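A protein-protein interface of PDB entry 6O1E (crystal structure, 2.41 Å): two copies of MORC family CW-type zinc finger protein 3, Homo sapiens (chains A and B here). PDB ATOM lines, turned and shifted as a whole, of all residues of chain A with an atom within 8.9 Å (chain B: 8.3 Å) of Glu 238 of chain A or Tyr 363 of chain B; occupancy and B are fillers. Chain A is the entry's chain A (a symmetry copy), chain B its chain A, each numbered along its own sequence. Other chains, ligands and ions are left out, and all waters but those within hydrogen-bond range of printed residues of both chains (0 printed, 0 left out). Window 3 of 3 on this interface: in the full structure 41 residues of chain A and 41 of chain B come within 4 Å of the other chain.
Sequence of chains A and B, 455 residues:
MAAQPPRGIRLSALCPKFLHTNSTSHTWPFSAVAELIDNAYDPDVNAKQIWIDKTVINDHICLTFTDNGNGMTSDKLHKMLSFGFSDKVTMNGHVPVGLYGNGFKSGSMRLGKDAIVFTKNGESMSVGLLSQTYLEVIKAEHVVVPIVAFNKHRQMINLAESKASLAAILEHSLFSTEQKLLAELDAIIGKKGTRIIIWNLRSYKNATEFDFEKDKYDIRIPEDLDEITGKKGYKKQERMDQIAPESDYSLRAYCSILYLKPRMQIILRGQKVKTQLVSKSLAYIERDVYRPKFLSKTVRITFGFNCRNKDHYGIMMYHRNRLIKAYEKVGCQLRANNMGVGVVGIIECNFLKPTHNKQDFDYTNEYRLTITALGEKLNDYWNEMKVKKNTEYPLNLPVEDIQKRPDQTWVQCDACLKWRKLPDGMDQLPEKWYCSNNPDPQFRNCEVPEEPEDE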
ATOM      1  N   THR A  27      -0.671  -1.713 -13.334  1.00  0.00           N
ATOM      2  CA  THR A  27      -0.025  -0.951 -12.269  1.00  0.00           C
ATOM      3  C   THR A  27      -0.058   0.542 -12.557  1.00  0.00           C
ATOM      4  O   THR A  27      -0.338   1.342 -11.668  1.00  0.00           O
ATOM      5  CB  THR A  27       1.411  -1.422 -12.095  1.00  0.00           C
ATOM      6  OG1 THR A  27       2.019  -1.554 -13.392  1.00  0.00           O
ATOM      7  CG2 THR A  27       1.423  -2.778 -11.398  1.00  0.00           C
ATOM      8  N   TRP A  28       0.214   0.910 -13.795  1.00  0.00           N
ATOM      9  CA  TRP A  28       0.092   2.280 -14.260  1.00  0.00           C
ATOM     10  C   TRP A  28      -1.362   2.558 -14.642  1.00  0.00           C
ATOM     11  O   TRP A  28      -1.910   1.861 -15.507  1.00  0.00           O
ATOM     12  CB  TRP A  28       1.027   2.450 -15.450  1.00  0.00           C
ATOM     13  CG  TRP A  28       1.231   3.805 -15.955  1.00  0.00           C
ATOM     14  CD1 TRP A  28       1.534   4.922 -15.235  1.00  0.00           C
ATOM     15  CD2 TRP A  28       1.191   4.206 -17.330  1.00  0.00           C
ATOM     16  NE1 TRP A  28       1.672   6.002 -16.080  1.00  0.00           N
ATOM     17  CE2 TRP A  28       1.466   5.587 -17.371  1.00  0.00           C
ATOM     18  CE3 TRP A  28       0.940   3.532 -18.525  1.00  0.00           C
ATOM     19  CZ2 TRP A  28       1.492   6.306 -18.564  1.00  0.00           C
ATOM     20  CZ3 TRP A  28       0.968   4.249 -19.712  1.00  0.00           C
ATOM     21  CH2 TRP A  28       1.237   5.620 -19.722  1.00  0.00           C
ATOM     22  N   ILE A 221      -1.282  12.334 -13.102  1.00  0.00           N
ATOM     23  CA  ILE A 221      -0.855  11.512 -11.973  1.00  0.00           C
ATOM     24  C   ILE A 221      -0.001  12.383 -11.067  1.00  0.00           C
ATOM     25  O   ILE A 221       0.918  13.055 -11.561  1.00  0.00           O
ATOM     26  CB  ILE A 221      -0.075  10.271 -12.437  1.00  0.00           C
ATOM     27  CG1 ILE A 221      -1.007   9.302 -13.177  1.00  0.00           C
ATOM     28  CG2 ILE A 221       0.600   9.587 -11.258  1.00  0.00           C
ATOM     29  CD1 ILE A 221      -0.256   8.233 -13.951  1.00  0.00           C
ATOM     30  N   LYS A 235       6.798   9.686 -13.255  1.00  0.00           N
ATOM     31  CA  LYS A 235       8.018   8.871 -13.297  1.00  0.00           C
ATOM     32  C   LYS A 235       7.733   7.370 -13.044  1.00  0.00           C
ATOM     33  O   LYS A 235       7.209   7.015 -11.986  1.00  0.00           O
ATOM     34  CB  LYS A 235       9.052   9.379 -12.265  1.00  0.00           C
ATOM     35  CG  LYS A 235       9.537  10.841 -12.394  1.00  0.00           C
ATOM     36  CD  LYS A 235       8.526  11.877 -11.876  1.00  0.00           C
ATOM     37  CE  LYS A 235       8.745  13.255 -12.507  1.00  0.00           C
ATOM     38  NZ  LYS A 235       7.852  14.298 -11.941  1.00  0.00           N
ATOM     39  N   LYS A 236       8.072   6.504 -14.012  1.00  0.00           N
ATOM     40  CA  LYS A 236       8.014   5.051 -13.838  1.00  0.00           C
ATOM     41  C   LYS A 236       9.334   4.417 -14.269  1.00  0.00           C
ATOM     42  O   LYS A 236      10.099   4.997 -15.047  1.00  0.00           O
ATOM     43  CB  LYS A 236       6.886   4.377 -14.649  1.00  0.00           C
ATOM     44  CG  LYS A 236       5.588   5.150 -14.796  1.00  0.00           C
ATOM     45  CD  LYS A 236       4.775   4.558 -15.968  1.00  0.00           C
ATOM     46  CE  LYS A 236       5.584   4.474 -17.280  1.00  0.00           C
ATOM     47  NZ  LYS A 236       5.010   3.507 -18.293  1.00  0.00           N
ATOM     48  N   GLN A 237       9.595   3.213 -13.741  1.00  0.00           N
ATOM     49  CA  GLN A 237      10.716   2.359 -14.142  1.00  0.00           C
ATOM     50  C   GLN A 237      12.087   2.937 -13.781  1.00  0.00           C
ATOM     51  O   GLN A 237      13.062   2.189 -13.659  1.00  0.00           O
ATOM     52  CB  GLN A 237      10.608   2.053 -15.654  1.00  0.00           C
ATOM     53  CG  GLN A 237      11.769   1.275 -16.347  1.00  0.00           C
ATOM     54  CD  GLN A 237      12.936   2.137 -16.849  1.00  0.00           C
ATOM     55  OE1 GLN A 237      13.148   3.264 -16.406  1.00  0.00           O
ATOM     56  NE2 GLN A 237      13.682   1.598 -17.814  1.00  0.00           N
ATOM     57  N   GLU A 238      12.178   4.251 -13.572  1.00  0.00           N
ATOM     58  CA  GLU A 238      13.474   4.934 -13.494  1.00  0.00           C
ATOM     59  C   GLU A 238      13.870   5.370 -12.077  1.00  0.00           C
ATOM     60  O   GLU A 238      13.212   6.204 -11.449  1.00  0.00           O
ATOM     61  CB  GLU A 238      13.466   6.150 -14.421  1.00  0.00           C
ATOM     62  CG  GLU A 238      14.260   5.955 -15.700  1.00  0.00           C
ATOM     63  CD  GLU A 238      15.735   5.798 -15.429  1.00  0.00           C
ATOM     64  OE1 GLU A 238      16.401   6.823 -15.167  1.00  0.00           O
ATOM     65  OE2 GLU A 238      16.224   4.648 -15.456  1.00  0.00           O
ATOM     66  N   GLN A 242      16.655   9.524 -15.054  1.00  0.00           N
ATOM     67  CA  GLN A 242      16.269  10.539 -16.041  1.00  0.00           C
ATOM     68  C   GLN A 242      15.020  11.309 -15.508  1.00  0.00           C
ATOM     69  O   GLN A 242      14.559  11.075 -14.376  1.00  0.00           O
ATOM     70  CB  GLN A 242      16.037   9.892 -17.440  1.00  0.00           C
ATOM     71  CG  GLN A 242      15.277  10.734 -18.516  1.00  0.00           C
ATOM     72  CD  GLN A 242      15.970  10.827 -19.885  1.00  0.00           C
ATOM     73  OE1 GLN A 242      16.353   9.820 -20.483  1.00  0.00           O
ATOM     74  NE2 GLN A 242      16.177  12.058 -20.355  1.00  0.00           N
ATOM     75  N   ILE A 243      14.559  12.308 -16.288  1.00  0.00           N
ATOM     76  CA  ILE A 243      13.321  13.063 -16.108  1.00  0.00           C
ATOM     77  C   ILE A 243      12.179  12.254 -16.711  1.00  0.00           C
ATOM     78  O   ILE A 243      12.360  11.545 -17.705  1.00  0.00           O
ATOM     79  CB  ILE A 243      13.443  14.445 -16.798  1.00  0.00           C
ATOM     80  CG1 ILE A 243      14.835  15.063 -16.568  1.00  0.00           C
ATOM     81  CG2 ILE A 243      12.308  15.385 -16.370  1.00  0.00           C
ATOM     82  CD1 ILE A 243      15.850  14.736 -17.679  1.00  0.00           C
ATOM     83  N   ALA A 244      10.986  12.369 -16.138  1.00  0.00           N
ATOM     84  CA  ALA A 244       9.842  11.641 -16.699  1.00  0.00           C
ATOM     85  C   ALA A 244       9.330  12.330 -17.961  1.00  0.00           C
ATOM     86  O   ALA A 244       9.080  13.540 -17.931  1.00  0.00           O
ATOM     87  CB  ALA A 244       8.700  11.553 -15.695  1.00  0.00           C
ATOM     88  N   PRO A 245       9.143  11.599 -19.070  1.00  0.00           N
ATOM     89  CA  PRO A 245       8.379  12.152 -20.199  1.00  0.00           C
ATOM     90  C   PRO A 245       6.961  12.500 -19.772  1.00  0.00           C
ATOM     91  O   PRO A 245       6.381  11.861 -18.895  1.00  0.00           O
ATOM     92  CB  PRO A 245       8.374  11.009 -21.219  1.00  0.00           C
ATOM     93  CG  PRO A 245       8.496   9.768 -20.371  1.00  0.00           C
ATOM     94  CD  PRO A 245       9.445  10.168 -19.266  1.00  0.00           C
ATOM     95  N   ASP A 248       4.185   9.879 -19.115  1.00  0.00           N
ATOM     96  CA  ASP A 248       4.074   9.081 -17.897  1.00  0.00           C
ATOM     97  C   ASP A 248       3.051   9.662 -16.918  1.00  0.00           C
ATOM     98  O   ASP A 248       2.485   8.919 -16.112  1.00  0.00           O
ATOM     99  CB  ASP A 248       5.436   8.954 -17.203  1.00  0.00           C
ATOM    100  CG  ASP A 248       6.368   7.949 -17.886  1.00  0.00           C
ATOM    101  OD1 ASP A 248       6.030   7.408 -18.975  1.00  0.00           O
ATOM    102  OD2 ASP A 248       7.457   7.705 -17.326  1.00  0.00           O
ATOM    103  N   TYR A 327      10.279   5.779 -25.637  1.00  0.00           N
ATOM    104  CA  TYR A 327      11.534   6.357 -25.153  1.00  0.00           C
ATOM    105  C   TYR A 327      12.429   5.281 -24.541  1.00  0.00           C
ATOM    106  O   TYR A 327      12.969   5.434 -23.439  1.00  0.00           O
ATOM    107  CB  TYR A 327      11.271   7.487 -24.150  1.00  0.00           C
ATOM    108  CG  TYR A 327      10.211   8.468 -24.613  1.00  0.00           C
ATOM    109  CD1 TYR A 327       9.001   8.566 -23.953  1.00  0.00           C
ATOM    110  CD2 TYR A 327      10.437   9.316 -25.705  1.00  0.00           C
ATOM    111  CE1 TYR A 327       8.016   9.451 -24.370  1.00  0.00           C
ATOM    112  CE2 TYR A 327       9.454  10.217 -26.132  1.00  0.00           C
ATOM    113  CZ  TYR A 327       8.246  10.276 -25.450  1.00  0.00           C
ATOM    114  OH  TYR A 327       7.259  11.155 -25.838  1.00  0.00           O
ATOM    115  N   GLU A 328      12.574   4.179 -25.261  1.00  0.00           N
ATOM    116  CA  GLU A 328      13.503   3.130 -24.872  1.00  0.00           C
ATOM    117  C   GLU A 328      14.874   3.485 -25.448  1.00  0.00           C
ATOM    118  O   GLU A 328      15.031   3.596 -26.672  1.00  0.00           O
ATOM    119  CB  GLU A 328      12.999   1.771 -25.369  1.00  0.00           C
ATOM    120  CG  GLU A 328      13.897   0.577 -25.029  1.00  0.00           C
ATOM    121  CD  GLU A 328      14.010   0.314 -23.508  1.00  0.00           C
ATOM    122  OE1 GLU A 328      12.945   0.219 -22.839  1.00  0.00           O
ATOM    123  OE2 GLU A 328      15.158   0.196 -22.986  1.00  0.00           O
ATOM    124  N   LYS A 329      15.853   3.708 -24.579  1.00  0.00           N
ATOM    125  CA  LYS A 329      17.187   4.064 -25.047  1.00  0.00           C
ATOM    126  C   LYS A 329      17.903   2.834 -25.597  1.00  0.00           C
ATOM    127  O   LYS A 329      17.793   1.730 -25.052  1.00  0.00           O
ATOM    128  CB  LYS A 329      18.000   4.705 -23.922  1.00  0.00           C
ATOM    129  CG  LYS A 329      17.170   5.511 -22.939  1.00  0.00           C
ATOM    130  CD  LYS A 329      16.881   6.956 -23.413  1.00  0.00           C
ATOM    131  CE  LYS A 329      15.575   7.454 -22.750  1.00  0.00           C
ATOM    132  NZ  LYS A 329      15.243   8.890 -22.922  1.00  0.00           N
ATOM    133  N   LEU A 334      22.578   4.131 -24.245  1.00  0.00           N
ATOM    134  CA  LEU A 334      22.709   3.385 -22.992  1.00  0.00           C
ATOM    135  C   LEU A 334      24.058   3.625 -22.328  1.00  0.00           C
ATOM    136  O   LEU A 334      24.138   3.627 -21.098  1.00  0.00           O
ATOM    137  CB  LEU A 334      22.532   1.884 -23.231  1.00  0.00           C
ATOM    138  CG  LEU A 334      21.163   1.411 -23.705  1.00  0.00           C
ATOM    139  CD1 LEU A 334      21.269  -0.019 -24.261  1.00  0.00           C
ATOM    140  CD2 LEU A 334      20.127   1.524 -22.584  1.00  0.00           C
ATOM    141  N   ASN A 337      24.692   9.591 -21.035  1.00  0.00           N
ATOM    142  CA  ASN A 337      23.785  10.669 -21.419  1.00  0.00           C
ATOM    143  C   ASN A 337      24.455  11.745 -22.278  1.00  0.00           C
ATOM    144  O   ASN A 337      23.942  12.867 -22.342  1.00  0.00           O
ATOM    145  CB  ASN A 337      23.168  11.322 -20.176  1.00  0.00           C
ATOM    146  CG  ASN A 337      22.504  10.319 -19.244  1.00  0.00           C
ATOM    147  OD1 ASN A 337      22.431   9.125 -19.539  1.00  0.00           O
ATOM    148  ND2 ASN A 337      22.010  10.807 -18.106  1.00  0.00           N
ATOM    149  N   LYS B 325      12.194 -10.468  -5.853  1.00  0.00           N
ATOM    150  CA  LYS B 325      13.224  -9.898  -6.725  1.00  0.00           C
ATOM    151  C   LYS B 325      14.566 -10.393  -6.233  1.00  0.00           C
ATOM    152  O   LYS B 325      14.859 -10.278  -5.037  1.00  0.00           O
ATOM    153  CB  LYS B 325      13.254  -8.356  -6.668  1.00  0.00           C
ATOM    154  CG  LYS B 325      12.360  -7.612  -7.637  1.00  0.00           C
ATOM    155  CD  LYS B 325      12.434  -6.103  -7.359  1.00  0.00           C
ATOM    156  CE  LYS B 325      12.352  -5.295  -8.635  1.00  0.00           C
ATOM    157  NZ  LYS B 325      13.428  -5.717  -9.569  1.00  0.00           N
ATOM    158  N   LEU B 352       5.714  -3.416   1.066  1.00  0.00           N
ATOM    159  CA  LEU B 352       5.605  -3.168  -0.366  1.00  0.00           C
ATOM    160  C   LEU B 352       4.557  -4.096  -0.980  1.00  0.00           C
ATOM    161  O   LEU B 352       4.133  -5.080  -0.371  1.00  0.00           O
ATOM    162  CB  LEU B 352       6.960  -3.349  -1.047  1.00  0.00           C
ATOM    163  CG  LEU B 352       8.098  -2.441  -0.558  1.00  0.00           C
ATOM    164  CD1 LEU B 352       9.421  -2.738  -1.263  1.00  0.00           C
ATOM    165  CD2 LEU B 352       7.710  -0.977  -0.738  1.00  0.00           C
ATOM    166  N   LYS B 353       4.133  -3.774  -2.209  1.00  0.00           N
ATOM    167  CA  LYS B 353       3.062  -4.524  -2.862  1.00  0.00           C
ATOM    168  C   LYS B 353       3.620  -5.399  -3.977  1.00  0.00           C
ATOM    169  O   LYS B 353       4.014  -4.876  -5.037  1.00  0.00           O
ATOM    170  CB  LYS B 353       1.988  -3.587  -3.423  1.00  0.00           C
ATOM    171  CG  LYS B 353       1.407  -2.590  -2.405  1.00  0.00           C
ATOM    172  CD  LYS B 353       0.848  -3.287  -1.154  1.00  0.00           C
ATOM    173  CE  LYS B 353       0.751  -2.319   0.031  1.00  0.00           C
ATOM    174  NZ  LYS B 353       0.689  -0.877  -0.413  1.00  0.00           N
ATOM    175  N   PRO B 354       3.630  -6.721  -3.813  1.00  0.00           N
ATOM    176  CA  PRO B 354       4.053  -7.584  -4.919  1.00  0.00           C
ATOM    177  C   PRO B 354       3.090  -7.440  -6.086  1.00  0.00           C
ATOM    178  O   PRO B 354       1.880  -7.290  -5.905  1.00  0.00           O
ATOM    179  CB  PRO B 354       4.023  -9.004  -4.317  1.00  0.00           C
ATOM    180  CG  PRO B 354       3.833  -8.820  -2.841  1.00  0.00           C
ATOM    181  CD  PRO B 354       3.163  -7.483  -2.648  1.00  0.00           C
ATOM    182  N   THR B 355       3.647  -7.459  -7.293  1.00  0.00           N
ATOM    183  CA  THR B 355       2.869  -7.469  -8.524  1.00  0.00           C
ATOM    184  C   THR B 355       3.483  -8.481  -9.480  1.00  0.00           C
ATOM    185  O   THR B 355       4.545  -9.043  -9.213  1.00  0.00           O
ATOM    186  CB  THR B 355       2.856  -6.094  -9.209  1.00  0.00           C
ATOM    187  OG1 THR B 355       4.208  -5.730  -9.513  1.00  0.00           O
ATOM    188  CG2 THR B 355       2.199  -5.013  -8.319  1.00  0.00           C
ATOM    189  N   HIS B 356       2.807  -8.683 -10.617  1.00  0.00           N
ATOM    190  CA  HIS B 356       3.280  -9.532 -11.720  1.00  0.00           C
ATOM    191  C   HIS B 356       3.500 -10.970 -11.248  1.00  0.00           C
ATOM    192  O   HIS B 356       4.580 -11.539 -11.423  1.00  0.00           O
ATOM    193  CB  HIS B 356       4.571  -8.979 -12.348  1.00  0.00           C
ATOM    194  CG  HIS B 356       4.422  -7.645 -13.023  1.00  0.00           C
ATOM    195  ND1 HIS B 356       3.216  -6.985 -13.144  1.00  0.00           N
ATOM    196  CD2 HIS B 356       5.348  -6.840 -13.605  1.00  0.00           C
ATOM    197  CE1 HIS B 356       3.404  -5.836 -13.770  1.00  0.00           C
ATOM    198  NE2 HIS B 356       4.688  -5.724 -14.063  1.00  0.00           N
ATOM    199  N   ASP B 360       7.645  -8.986  -8.888  1.00  0.00           N
ATOM    200  CA  ASP B 360       8.068  -7.593  -8.850  1.00  0.00           C
ATOM    201  C   ASP B 360       7.262  -6.877  -7.767  1.00  0.00           C
ATOM    202  O   ASP B 360       6.319  -7.431  -7.196  1.00  0.00           O
ATOM    203  CB  ASP B 360       7.895  -6.927 -10.225  1.00  0.00           C
ATOM    204  CG  ASP B 360       8.914  -5.799 -10.484  1.00  0.00           C
ATOM    205  OD1 ASP B 360       9.195  -5.523 -11.678  1.00  0.00           O
ATOM    206  OD2 ASP B 360       9.425  -5.182  -9.509  1.00  0.00           O
ATOM    207  N   PHE B 361       7.653  -5.640  -7.483  1.00  0.00           N
ATOM    208  CA  PHE B 361       6.920  -4.774  -6.567  1.00  0.00           C
ATOM    209  C   PHE B 361       6.294  -3.623  -7.339  1.00  0.00           C
ATOM    210  O   PHE B 361       6.823  -3.184  -8.364  1.00  0.00           O
ATOM    211  CB  PHE B 361       7.832  -4.216  -5.471  1.00  0.00           C
ATOM    212  CG  PHE B 361       8.245  -5.235  -4.472  1.00  0.00           C
ATOM    213  CD1 PHE B 361       7.324  -5.770  -3.591  1.00  0.00           C
ATOM    214  CD2 PHE B 361       9.553  -5.681  -4.422  1.00  0.00           C
ATOM    215  CE1 PHE B 361       7.710  -6.710  -2.662  1.00  0.00           C
ATOM    216  CE2 PHE B 361       9.929  -6.624  -3.513  1.00  0.00           C
ATOM    217  CZ  PHE B 361       9.009  -7.136  -2.626  1.00  0.00           C
ATOM    218  N   ASP B 362       5.150  -3.156  -6.860  1.00  0.00           N
ATOM    219  CA  ASP B 362       4.575  -1.952  -7.438  1.00  0.00           C
ATOM    220  C   ASP B 362       5.572  -0.804  -7.311  1.00  0.00           C
ATOM    221  O   ASP B 362       6.144  -0.572  -6.244  1.00  0.00           O
ATOM    222  CB  ASP B 362       3.260  -1.606  -6.742  1.00  0.00           C
ATOM    223  CG  ASP B 362       2.431  -0.579  -7.522  1.00  0.00           C
ATOM    224  OD1 ASP B 362       2.711  -0.362  -8.725  1.00  0.00           O
ATOM    225  OD2 ASP B 362       1.489   0.005  -6.930  1.00  0.00           O
ATOM    226  N   TYR B 363       5.796  -0.090  -8.411  1.00  0.00           N
ATOM    227  CA  TYR B 363       6.838   0.932  -8.435  1.00  0.00           C
ATOM    228  C   TYR B 363       6.335   2.236  -7.790  1.00  0.00           C
ATOM    229  O   TYR B 363       6.149   3.268  -8.436  1.00  0.00           O
ATOM    230  CB  TYR B 363       7.323   1.137  -9.864  1.00  0.00           C
ATOM    231  CG  TYR B 363       8.505   2.065  -9.948  1.00  0.00           C
ATOM    232  CD1 TYR B 363       9.774   1.635  -9.566  1.00  0.00           C
ATOM    233  CD2 TYR B 363       8.358   3.376 -10.405  1.00  0.00           C
ATOM    234  CE1 TYR B 363      10.868   2.478  -9.629  1.00  0.00           C
ATOM    235  CE2 TYR B 363       9.451   4.230 -10.476  1.00  0.00           C
ATOM    236  CZ  TYR B 363      10.702   3.773 -10.083  1.00  0.00           C
ATOM    237  OH  TYR B 363      11.788   4.612 -10.147  1.00  0.00           O
ATOM    238  N   THR B 364       6.158   2.188  -6.462  1.00  0.00           N
ATOM    239  CA  THR B 364       5.625   3.313  -5.710  1.00  0.00           C
ATOM    240  C   THR B 364       6.743   4.202  -5.164  1.00  0.00           C
ATOM    241  O   THR B 364       7.940   3.964  -5.357  1.00  0.00           O
ATOM    242  CB  THR B 364       4.768   2.831  -4.546  1.00  0.00           C
ATOM    243  OG1 THR B 364       5.563   1.973  -3.711  1.00  0.00           O
ATOM    244  CG2 THR B 364       3.538   2.083  -5.036  1.00  0.00           C
ATOM    245  N   ASN B 365       6.336   5.245  -4.443  1.00  0.00           N
ATOM    246  CA  ASN B 365       7.313   6.099  -3.788  1.00  0.00           C
ATOM    247  C   ASN B 365       8.015   5.355  -2.658  1.00  0.00           C
ATOM    248  O   ASN B 365       9.233   5.469  -2.492  1.00  0.00           O
ATOM    249  CB  ASN B 365       6.629   7.359  -3.264  1.00  0.00           C
ATOM    250  CG  ASN B 365       7.598   8.497  -3.075  1.00  0.00           C
ATOM    251  OD1 ASN B 365       8.330   8.854  -4.005  1.00  0.00           O
ATOM    252  ND2 ASN B 365       7.634   9.066  -1.863  1.00  0.00           N
ATOM    253  N   GLU B 366       7.255   4.595  -1.866  1.00  0.00           N
ATOM    254  CA  GLU B 366       7.860   3.772  -0.826  1.00  0.00           C
ATOM    255  C   GLU B 366       8.875   2.808  -1.417  1.00  0.00           C
ATOM    256  O   GLU B 366       9.976   2.657  -0.878  1.00  0.00           O
ATOM    257  CB  GLU B 366       6.770   3.048  -0.044  1.00  0.00           C
ATOM    258  CG  GLU B 366       5.886   4.085   0.689  1.00  0.00           C
ATOM    259  CD  GLU B 366       4.557   3.543   1.168  1.00  0.00           C
ATOM    260  OE1 GLU B 366       4.539   2.626   2.023  1.00  0.00           O
ATOM    261  OE2 GLU B 366       3.519   4.043   0.682  1.00  0.00           O
ATOM    262  N   TYR B 367       8.571   2.213  -2.572  1.00  0.00           N
ATOM    263  CA  TYR B 367       9.588   1.400  -3.221  1.00  0.00           C
ATOM    264  C   TYR B 367      10.841   2.216  -3.513  1.00  0.00           C
ATOM    265  O   TYR B 367      11.960   1.757  -3.248  1.00  0.00           O
ATOM    266  CB  TYR B 367       9.061   0.769  -4.509  1.00  0.00           C
ATOM    267  CG  TYR B 367      10.111  -0.081  -5.187  1.00  0.00           C
ATOM    268  CD1 TYR B 367      10.348  -1.387  -4.765  1.00  0.00           C
ATOM    269  CD2 TYR B 367      10.893   0.431  -6.227  1.00  0.00           C
ATOM    270  CE1 TYR B 367      11.315  -2.178  -5.369  1.00  0.00           C
ATOM    271  CE2 TYR B 367      11.868  -0.344  -6.839  1.00  0.00           C
ATOM    272  CZ  TYR B 367      12.074  -1.653  -6.396  1.00  0.00           C
ATOM    273  OH  TYR B 367      13.035  -2.435  -6.978  1.00  0.00           O
ATOM    274  N   ARG B 368      10.682   3.424  -4.060  1.00  0.00           N
ATOM    275  CA  ARG B 368      11.855   4.201  -4.468  1.00  0.00           C
ATOM    276  C   ARG B 368      12.692   4.619  -3.264  1.00  0.00           C
ATOM    277  O   ARG B 368      13.929   4.602  -3.326  1.00  0.00           O
ATOM    278  CB  ARG B 368      11.425   5.421  -5.283  1.00  0.00           C
ATOM    279  CG  ARG B 368      11.191   5.108  -6.761  1.00  0.00           C
ATOM    280  CD  ARG B 368      11.017   6.386  -7.587  1.00  0.00           C
ATOM    281  NE  ARG B 368      10.011   7.253  -6.987  1.00  0.00           N
ATOM    282  CZ  ARG B 368       8.704   7.183  -7.243  1.00  0.00           C
ATOM    283  NH1 ARG B 368       8.238   6.288  -8.115  1.00  0.00           N
ATOM    284  NH2 ARG B 368       7.862   8.011  -6.622  1.00  0.00           N
ATOM    285  N   LEU B 369      12.042   4.972  -2.153  1.00  0.00           N
ATOM    286  CA  LEU B 369      12.783   5.348  -0.954  1.00  0.00           C
ATOM    287  C   LEU B 369      13.505   4.147  -0.345  1.00  0.00           C
ATOM    288  O   LEU B 369      14.644   4.271   0.122  1.00  0.00           O
ATOM    289  CB  LEU B 369      11.830   5.975   0.065  1.00  0.00           C
ATOM    290  CG  LEU B 369      11.237   7.367  -0.235  1.00  0.00           C
ATOM    291  CD1 LEU B 369      10.078   7.657   0.685  1.00  0.00           C
ATOM    292  CD2 LEU B 369      12.286   8.469  -0.085  1.00  0.00           C
ATOM    293  N   ILE B 371      14.625   1.503  -2.006  1.00  0.00           N
ATOM    294  CA  ILE B 371      15.771   1.235  -2.872  1.00  0.00           C
ATOM    295  C   ILE B 371      16.898   2.227  -2.588  1.00  0.00           C
ATOM    296  O   ILE B 371      18.086   1.864  -2.567  1.00  0.00           O
ATOM    297  CB  ILE B 371      15.314   1.274  -4.343  1.00  0.00           C
ATOM    298  CG1 ILE B 371      14.546  -0.006  -4.700  1.00  0.00           C
ATOM    299  CG2 ILE B 371      16.472   1.536  -5.287  1.00  0.00           C
ATOM    300  CD1 ILE B 371      15.342  -1.316  -4.473  1.00  0.00           C
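OH of Tyr 363 of chain B is in hydrogen-bond range of O of Glu 238 of chain A (2.5 Å).
The backbone carbonyl oxygen (O) of Lys 353 of chain B sits at hydrogen-bond distance from the backbone NH (N) of Asp 362 of chain B (2.8 Å).
O of Asp 360 of chain B lies within hydrogen-bond range of N of Thr 355 of chain B (2.7 Å).
N of Gln 242 of chain A is in hydrogen-bond range of OE1 of Glu 238 of chain A (2.7 Å).
Thr 27 of chain A touches Thr 355 of chain B (CG2 to CG2, 3.9 Å).
CB of Thr 27 of chain A touches OD1 of Asp 362 of chain B, 3.8 Å away.
Lys 235 of chain A touches Tyr 363 of chain B.
CE2 of Tyr 363 of chain B touches CA of Lys 236 of chain A (3.7 Å).
Gln 237 of chain A touches Tyr 363 of chain B.
Of chain B, only Tyr 363 comes within 4 Å of Glu 238 of chain A.
Of chain A, only Lys 235 (3.9 Å), Lys 236 (3.7 Å), Gln 237 (3.4 Å) and Glu 238 (2.5 Å) come within 4 Å of Tyr 363 of chain B.
Asp 362 of chain B touches just one residue of chain A: Thr 27 (3.8 Å).
Of the printed residues of chain B, Lys 236 of chain A touches Tyr 363.
Of the printed residues of chain A, Thr 355 of chain B touches Thr 27 (3.9 Å).
Of the printed residues of chain B, Thr 27 of chain A touches Thr 355 and Asp 362.
Printed residues of chain B within 4 Å of Gln 237 of chain A: Tyr 363 (3.4 Å).
Of the printed residues of chain B, Lys 235 of chain A touches Tyr 363 (3.9 Å).
The nearest residue of chain A that does not touch Tyr 363 of chain B is Thr 27 of chain A (5.9 Å).
Among the printed residues, no Asp or Glu carboxylate lies within 4 Å of a Lys or Arg side-chain nitrogen of the other chain.
No position is printed for both chains.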
